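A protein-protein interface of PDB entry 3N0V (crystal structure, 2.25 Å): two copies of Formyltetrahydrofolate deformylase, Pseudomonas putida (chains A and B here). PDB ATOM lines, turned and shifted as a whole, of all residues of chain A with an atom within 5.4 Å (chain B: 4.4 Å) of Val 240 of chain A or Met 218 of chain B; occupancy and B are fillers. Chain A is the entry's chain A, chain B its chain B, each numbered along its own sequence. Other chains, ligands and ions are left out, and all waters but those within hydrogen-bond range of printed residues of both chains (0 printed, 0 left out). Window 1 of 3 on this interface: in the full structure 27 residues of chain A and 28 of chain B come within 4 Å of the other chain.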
ATOM      1  N   MET A 218     -29.628 -20.330 -15.456  1.00  0.00           N
ATOM      2  CA  MET A 218     -28.421 -20.718 -14.736  1.00  0.00           C
ATOM      3  C   MET A 218     -27.303 -19.712 -14.934  1.00  0.00           C
ATOM      4  O   MET A 218     -27.159 -19.153 -16.020  1.00  0.00           O
ATOM      5  CB  MET A 218     -27.844 -22.010 -15.280  1.00  0.00           C
ATOM      6  CG  MET A 218     -28.804 -23.081 -15.609  1.00  0.00           C
ATOM      7  SD  MET A 218     -27.745 -24.556 -16.277  1.00  0.00           S
ATOM      8  CE  MET A 218     -26.885 -23.761 -17.791  1.00  0.00           C
ATOM      9  N   VAL A 219     -26.463 -19.564 -13.912  1.00  0.00           N
ATOM     10  CA  VAL A 219     -25.177 -18.871 -14.032  1.00  0.00           C
ATOM     11  C   VAL A 219     -24.079 -19.852 -13.620  1.00  0.00           C
ATOM     12  O   VAL A 219     -24.313 -20.702 -12.772  1.00  0.00           O
ATOM     13  CB  VAL A 219     -25.146 -17.577 -13.183  1.00  0.00           C
ATOM     14  CG1 VAL A 219     -26.365 -16.717 -13.507  1.00  0.00           C
ATOM     15  CG2 VAL A 219     -25.100 -17.878 -11.710  1.00  0.00           C
ATOM     16  N   GLY A 220     -22.894 -19.750 -14.227  1.00  0.00           N
ATOM     17  CA  GLY A 220     -21.863 -20.789 -14.070  1.00  0.00           C
ATOM     18  C   GLY A 220     -20.476 -20.277 -13.733  1.00  0.00           C
ATOM     19  O   GLY A 220     -20.245 -19.070 -13.727  1.00  0.00           O
ATOM     20  N   ALA A 221     -19.553 -21.202 -13.443  1.00  0.00           N
ATOM     21  CA  ALA A 221     -18.166 -20.849 -13.131  1.00  0.00           C
ATOM     22  C   ALA A 221     -17.213 -21.981 -13.437  1.00  0.00           C
ATOM     23  O   ALA A 221     -17.585 -23.156 -13.345  1.00  0.00           O
ATOM     24  CB  ALA A 221     -18.036 -20.471 -11.690  1.00  0.00           C
ATOM     25  N   GLN A 238     -16.201 -27.318 -12.699  1.00  0.00           N
ATOM     26  CA  GLN A 238     -17.208 -26.388 -13.205  1.00  0.00           C
ATOM     27  C   GLN A 238     -18.499 -26.630 -12.448  1.00  0.00           C
ATOM     28  O   GLN A 238     -18.782 -27.753 -12.065  1.00  0.00           O
ATOM     29  CB  GLN A 238     -17.470 -26.597 -14.702  1.00  0.00           C
ATOM     30  CG  GLN A 238     -16.270 -26.422 -15.612  1.00  0.00           C
ATOM     31  CD  GLN A 238     -16.608 -26.692 -17.072  1.00  0.00           C
ATOM     32  OE1 GLN A 238     -16.992 -27.801 -17.440  1.00  0.00           O
ATOM     33  NE2 GLN A 238     -16.467 -25.678 -17.907  1.00  0.00           N
ATOM     34  N   GLY A 239     -19.294 -25.583 -12.265  1.00  0.00           N
ATOM     35  CA  GLY A 239     -20.604 -25.713 -11.623  1.00  0.00           C
ATOM     36  C   GLY A 239     -21.559 -24.625 -12.055  1.00  0.00           C
ATOM     37  O   GLY A 239     -21.146 -23.630 -12.656  1.00  0.00           O
ATOM     38  N   VAL A 240     -22.841 -24.822 -11.765  1.00  0.00           N
ATOM     39  CA  VAL A 240     -23.852 -23.806 -12.015  1.00  0.00           C
ATOM     40  C   VAL A 240     -24.753 -23.641 -10.812  1.00  0.00           C
ATOM     41  O   VAL A 240     -24.825 -24.508  -9.940  1.00  0.00           O
ATOM     42  CB  VAL A 240     -24.742 -24.130 -13.241  1.00  0.00           C
ATOM     43  CG1 VAL A 240     -23.896 -24.234 -14.503  1.00  0.00           C
ATOM     44  CG2 VAL A 240     -25.563 -25.402 -13.003  1.00  0.00           C
ATOM     45  N   GLU A 241     -25.420 -22.499 -10.784  1.00  0.00           N
ATOM     46  CA  GLU A 241     -26.395 -22.152  -9.765  1.00  0.00           C
ATOM     47  C   GLU A 241     -27.692 -21.810 -10.511  1.00  0.00           C
ATOM     48  O   GLU A 241     -27.665 -21.111 -11.537  1.00  0.00           O
ATOM     49  CB  GLU A 241     -25.892 -20.938  -8.970  1.00  0.00           C
ATOM     50  CG  GLU A 241     -26.571 -20.696  -7.648  1.00  0.00           C
ATOM     51  CD  GLU A 241     -26.086 -21.623  -6.559  1.00  0.00           C
ATOM     52  OE1 GLU A 241     -24.871 -21.639  -6.263  1.00  0.00           O
ATOM     53  OE2 GLU A 241     -26.924 -22.336  -5.984  1.00  0.00           O
ATOM     54  N   VAL A 242     -28.808 -22.342 -10.026  1.00  0.00           N
ATOM     55  CA  VAL A 242     -30.116 -22.038 -10.577  1.00  0.00           C
ATOM     56  C   VAL A 242     -30.446 -20.577 -10.298  1.00  0.00           C
ATOM     57  O   VAL A 242     -30.285 -20.112  -9.171  1.00  0.00           O
ATOM     58  CB  VAL A 242     -31.210 -22.947  -9.956  1.00  0.00           C
ATOM     59  CG1 VAL A 242     -32.598 -22.502 -10.385  1.00  0.00           C
ATOM     60  CG2 VAL A 242     -30.974 -24.421 -10.335  1.00  0.00           C
ATOM     61  N   ILE A 259     -21.359 -19.214  -6.915  1.00  0.00           N
ATOM     62  CA  ILE A 259     -20.890 -20.343  -7.712  1.00  0.00           C
ATOM     63  C   ILE A 259     -19.395 -20.234  -7.977  1.00  0.00           C
ATOM     64  O   ILE A 259     -18.710 -21.247  -8.121  1.00  0.00           O
ATOM     65  CB  ILE A 259     -21.698 -20.518  -9.032  1.00  0.00           C
ATOM     66  CG1 ILE A 259     -21.378 -21.874  -9.678  1.00  0.00           C
ATOM     67  CG2 ILE A 259     -21.459 -19.330 -10.022  1.00  0.00           C
ATOM     68  CD1 ILE A 259     -21.546 -23.069  -8.740  1.00  0.00           C
ATOM     69  N   LEU B 199     -19.676 -25.959 -23.093  1.00  0.00           N
ATOM     70  CA  LEU B 199     -18.746 -24.941 -22.614  1.00  0.00           C
ATOM     71  C   LEU B 199     -17.587 -24.788 -23.575  1.00  0.00           C
ATOM     72  O   LEU B 199     -17.312 -23.685 -24.035  1.00  0.00           O
ATOM     73  CB  LEU B 199     -18.238 -25.320 -21.224  1.00  0.00           C
ATOM     74  CG  LEU B 199     -19.359 -25.297 -20.180  1.00  0.00           C
ATOM     75  CD1 LEU B 199     -19.178 -26.384 -19.119  1.00  0.00           C
ATOM     76  CD2 LEU B 199     -19.474 -23.910 -19.553  1.00  0.00           C
ATOM     77  N   VAL B 216     -14.385 -30.668 -20.377  1.00  0.00           N
ATOM     78  CA  VAL B 216     -15.518 -30.113 -19.624  1.00  0.00           C
ATOM     79  C   VAL B 216     -15.970 -31.082 -18.539  1.00  0.00           C
ATOM     80  O   VAL B 216     -15.738 -32.282 -18.630  1.00  0.00           O
ATOM     81  CB  VAL B 216     -16.729 -29.746 -20.541  1.00  0.00           C
ATOM     82  CG1 VAL B 216     -16.346 -28.685 -21.545  1.00  0.00           C
ATOM     83  CG2 VAL B 216     -17.304 -30.978 -21.257  1.00  0.00           C
ATOM     84  N   LYS B 217     -16.596 -30.551 -17.495  1.00  0.00           N
ATOM     85  CA  LYS B 217     -17.072 -31.368 -16.373  1.00  0.00           C
ATOM     86  C   LYS B 217     -18.595 -31.311 -16.237  1.00  0.00           C
ATOM     87  O   LYS B 217     -19.141 -31.717 -15.201  1.00  0.00           O
ATOM     88  CB  LYS B 217     -16.421 -30.915 -15.059  1.00  0.00           C
ATOM     89  CG  LYS B 217     -14.896 -30.819 -15.082  1.00  0.00           C
ATOM     90  CD  LYS B 217     -14.182 -32.144 -15.370  1.00  0.00           C
ATOM     91  CE  LYS B 217     -12.667 -31.958 -15.358  1.00  0.00           C
ATOM     92  NZ  LYS B 217     -11.904 -33.168 -15.751  1.00  0.00           N
ATOM     93  N   MET B 218     -19.263 -30.779 -17.266  1.00  0.00           N
ATOM     94  CA  MET B 218     -20.721 -30.789 -17.377  1.00  0.00           C
ATOM     95  C   MET B 218     -21.129 -30.818 -18.841  1.00  0.00           C
ATOM     96  O   MET B 218     -20.384 -30.352 -19.704  1.00  0.00           O
ATOM     97  CB  MET B 218     -21.346 -29.525 -16.790  1.00  0.00           C
ATOM     98  CG  MET B 218     -20.723 -28.988 -15.541  1.00  0.00           C
ATOM     99  SD  MET B 218     -21.588 -27.339 -14.980  1.00  0.00           S
ATOM    100  CE  MET B 218     -21.157 -26.239 -16.465  1.00  0.00           C
ATOM    101  N   VAL B 219     -22.320 -31.356 -19.102  1.00  0.00           N
ATOM    102  CA  VAL B 219     -23.040 -31.103 -20.350  1.00  0.00           C
ATOM    103  C   VAL B 219     -24.393 -30.504 -20.005  1.00  0.00           C
ATOM    104  O   VAL B 219     -24.937 -30.765 -18.933  1.00  0.00           O
ATOM    105  CB  VAL B 219     -23.253 -32.369 -21.199  1.00  0.00           C
ATOM    106  CG1 VAL B 219     -21.917 -32.870 -21.740  1.00  0.00           C
ATOM    107  CG2 VAL B 219     -23.990 -33.454 -20.408  1.00  0.00           C
ATOM    108  N   VAL B 240     -28.033 -28.967 -16.388  1.00  0.00           N
ATOM    109  CA  VAL B 240     -26.767 -29.600 -16.711  1.00  0.00           C
ATOM    110  C   VAL B 240     -26.705 -30.966 -16.092  1.00  0.00           C
ATOM    111  O   VAL B 240     -27.494 -31.293 -15.212  1.00  0.00           O
ATOM    112  CB  VAL B 240     -25.555 -28.797 -16.207  1.00  0.00           C
ATOM    113  CG1 VAL B 240     -25.510 -27.403 -16.876  1.00  0.00           C
ATOM    114  CG2 VAL B 240     -25.571 -28.726 -14.655  1.00  0.00           C
ATOM    115  N   GLU B 241     -25.743 -31.747 -16.574  1.00  0.00           N
ATOM    116  CA  GLU B 241     -25.450 -33.076 -16.074  1.00  0.00           C
ATOM    117  C   GLU B 241     -23.952 -33.136 -15.813  1.00  0.00           C
ATOM    118  O   GLU B 241     -23.159 -32.775 -16.680  1.00  0.00           O
ATOM    119  CB  GLU B 241     -25.820 -34.123 -17.130  1.00  0.00           C
ATOM    120  CG  GLU B 241     -25.835 -35.560 -16.626  1.00  0.00           C
ATOM    121  CD  GLU B 241     -27.091 -35.891 -15.841  1.00  0.00           C
ATOM    122  OE1 GLU B 241     -28.185 -35.922 -16.447  1.00  0.00           O
ATOM    123  OE2 GLU B 241     -26.983 -36.127 -14.621  1.00  0.00           O
ATOM    124  N   VAL B 243     -20.306 -34.542 -15.570  1.00  0.00           N
ATOM    125  CA  VAL B 243     -19.475 -35.537 -16.262  1.00  0.00           C
ATOM    126  C   VAL B 243     -18.039 -35.442 -15.761  1.00  0.00           C
ATOM    127  O   VAL B 243     -17.671 -34.467 -15.105  1.00  0.00           O
ATOM    128  CB  VAL B 243     -19.499 -35.355 -17.801  1.00  0.00           C
ATOM    129  CG1 VAL B 243     -20.932 -35.431 -18.332  1.00  0.00           C
ATOM    130  CG2 VAL B 243     -18.841 -34.044 -18.206  1.00  0.00           C
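Val 240 of chain B touches Met 218 of chain A.
CD1 of Leu 199 of chain B touches NE2 of Gln 238 of chain A (3.1 Å).
Val 216 of chain B touches Gln 238 of chain A.
Gln 238 of chain A touches Met 218 of chain B (OE1 to N, 3.7 Å).
CA of Gly 239 of chain A touches SD of Met 218 of chain B, 3.9 Å away.
Met 218 of chain B touches Val 240 of chain A (SD to CG1, 3.9 Å).
Val 240 of chain B touches Val 240 of chain A (CG2 to CG2, 3.7 Å).
N of Lys 217 of chain B lies within hydrogen-bond range of OE1 of Gln 238 of chain A, at 2.8 Å.
Of the 8 printed residues of chain B, 5 touch a printed residue of chain A.
Printed residues of chain B that touch a printed residue of chain A: Leu 199, Val 216, Lys 217, Met 218 and Val 240.
Hydrophobic or aromatic side chains of chain B that line the printed part of chain A: Leu 199, Val 216, Met 218 and Val 240.
Printed residues of chain A that touch a printed residue of chain B: Met 218, Gln 238, Gly 239 and Val 240.
Among the printed residues, 8 pairs touch across the chains.
The backbone NH (N) of Ala 221 of chain A lies within hydrogen-bond range of the backbone carbonyl oxygen (O) of Gly 239 of chain A, at 3.0 Å.
The backbone NH (N) of Val 243 of chain B is in hydrogen-bond range of the backbone carbonyl oxygen (O) of Lys 217 of chain B (3.1 Å).
Printed residues of chain B within 4 Å of Met 218 of chain A: Val 240.
Of the printed residues of chain B, Gln 238 of chain A touches Leu 199 (3.1 Å), Val 216 (3.5 Å), Lys 217 (2.8 Å) and Met 218 (3.7 Å).
Of the printed residues of chain B, Val 240 of chain A touches Met 218 and Val 240.
Printed residues of chain A within 4 Å of Leu 199 of chain B: Gln 238.
Of the printed residues of chain A, Val 216 of chain B touches Gln 238 (3.5 Å).
Of the printed residues of chain A, Lys 217 of chain B touches Gln 238.
The nearest printed residue of chain B that does not touch Val 240 of chain A is Leu 199 of chain B (6.7 Å).
The nearest printed residue of chain A that does not touch Met 218 of chain B is Ala 221 of chain A (5.7 Å).
Met 218 of chain A touches Val 240 of chain B, and with the chains exchanged Val 240 of chain A touches Met 218 of chain B.
Val 240 of chain B touches its own counterpart, Val 240 of chain A.
Positions printed for both chains: 218, 219, 240 and 241.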
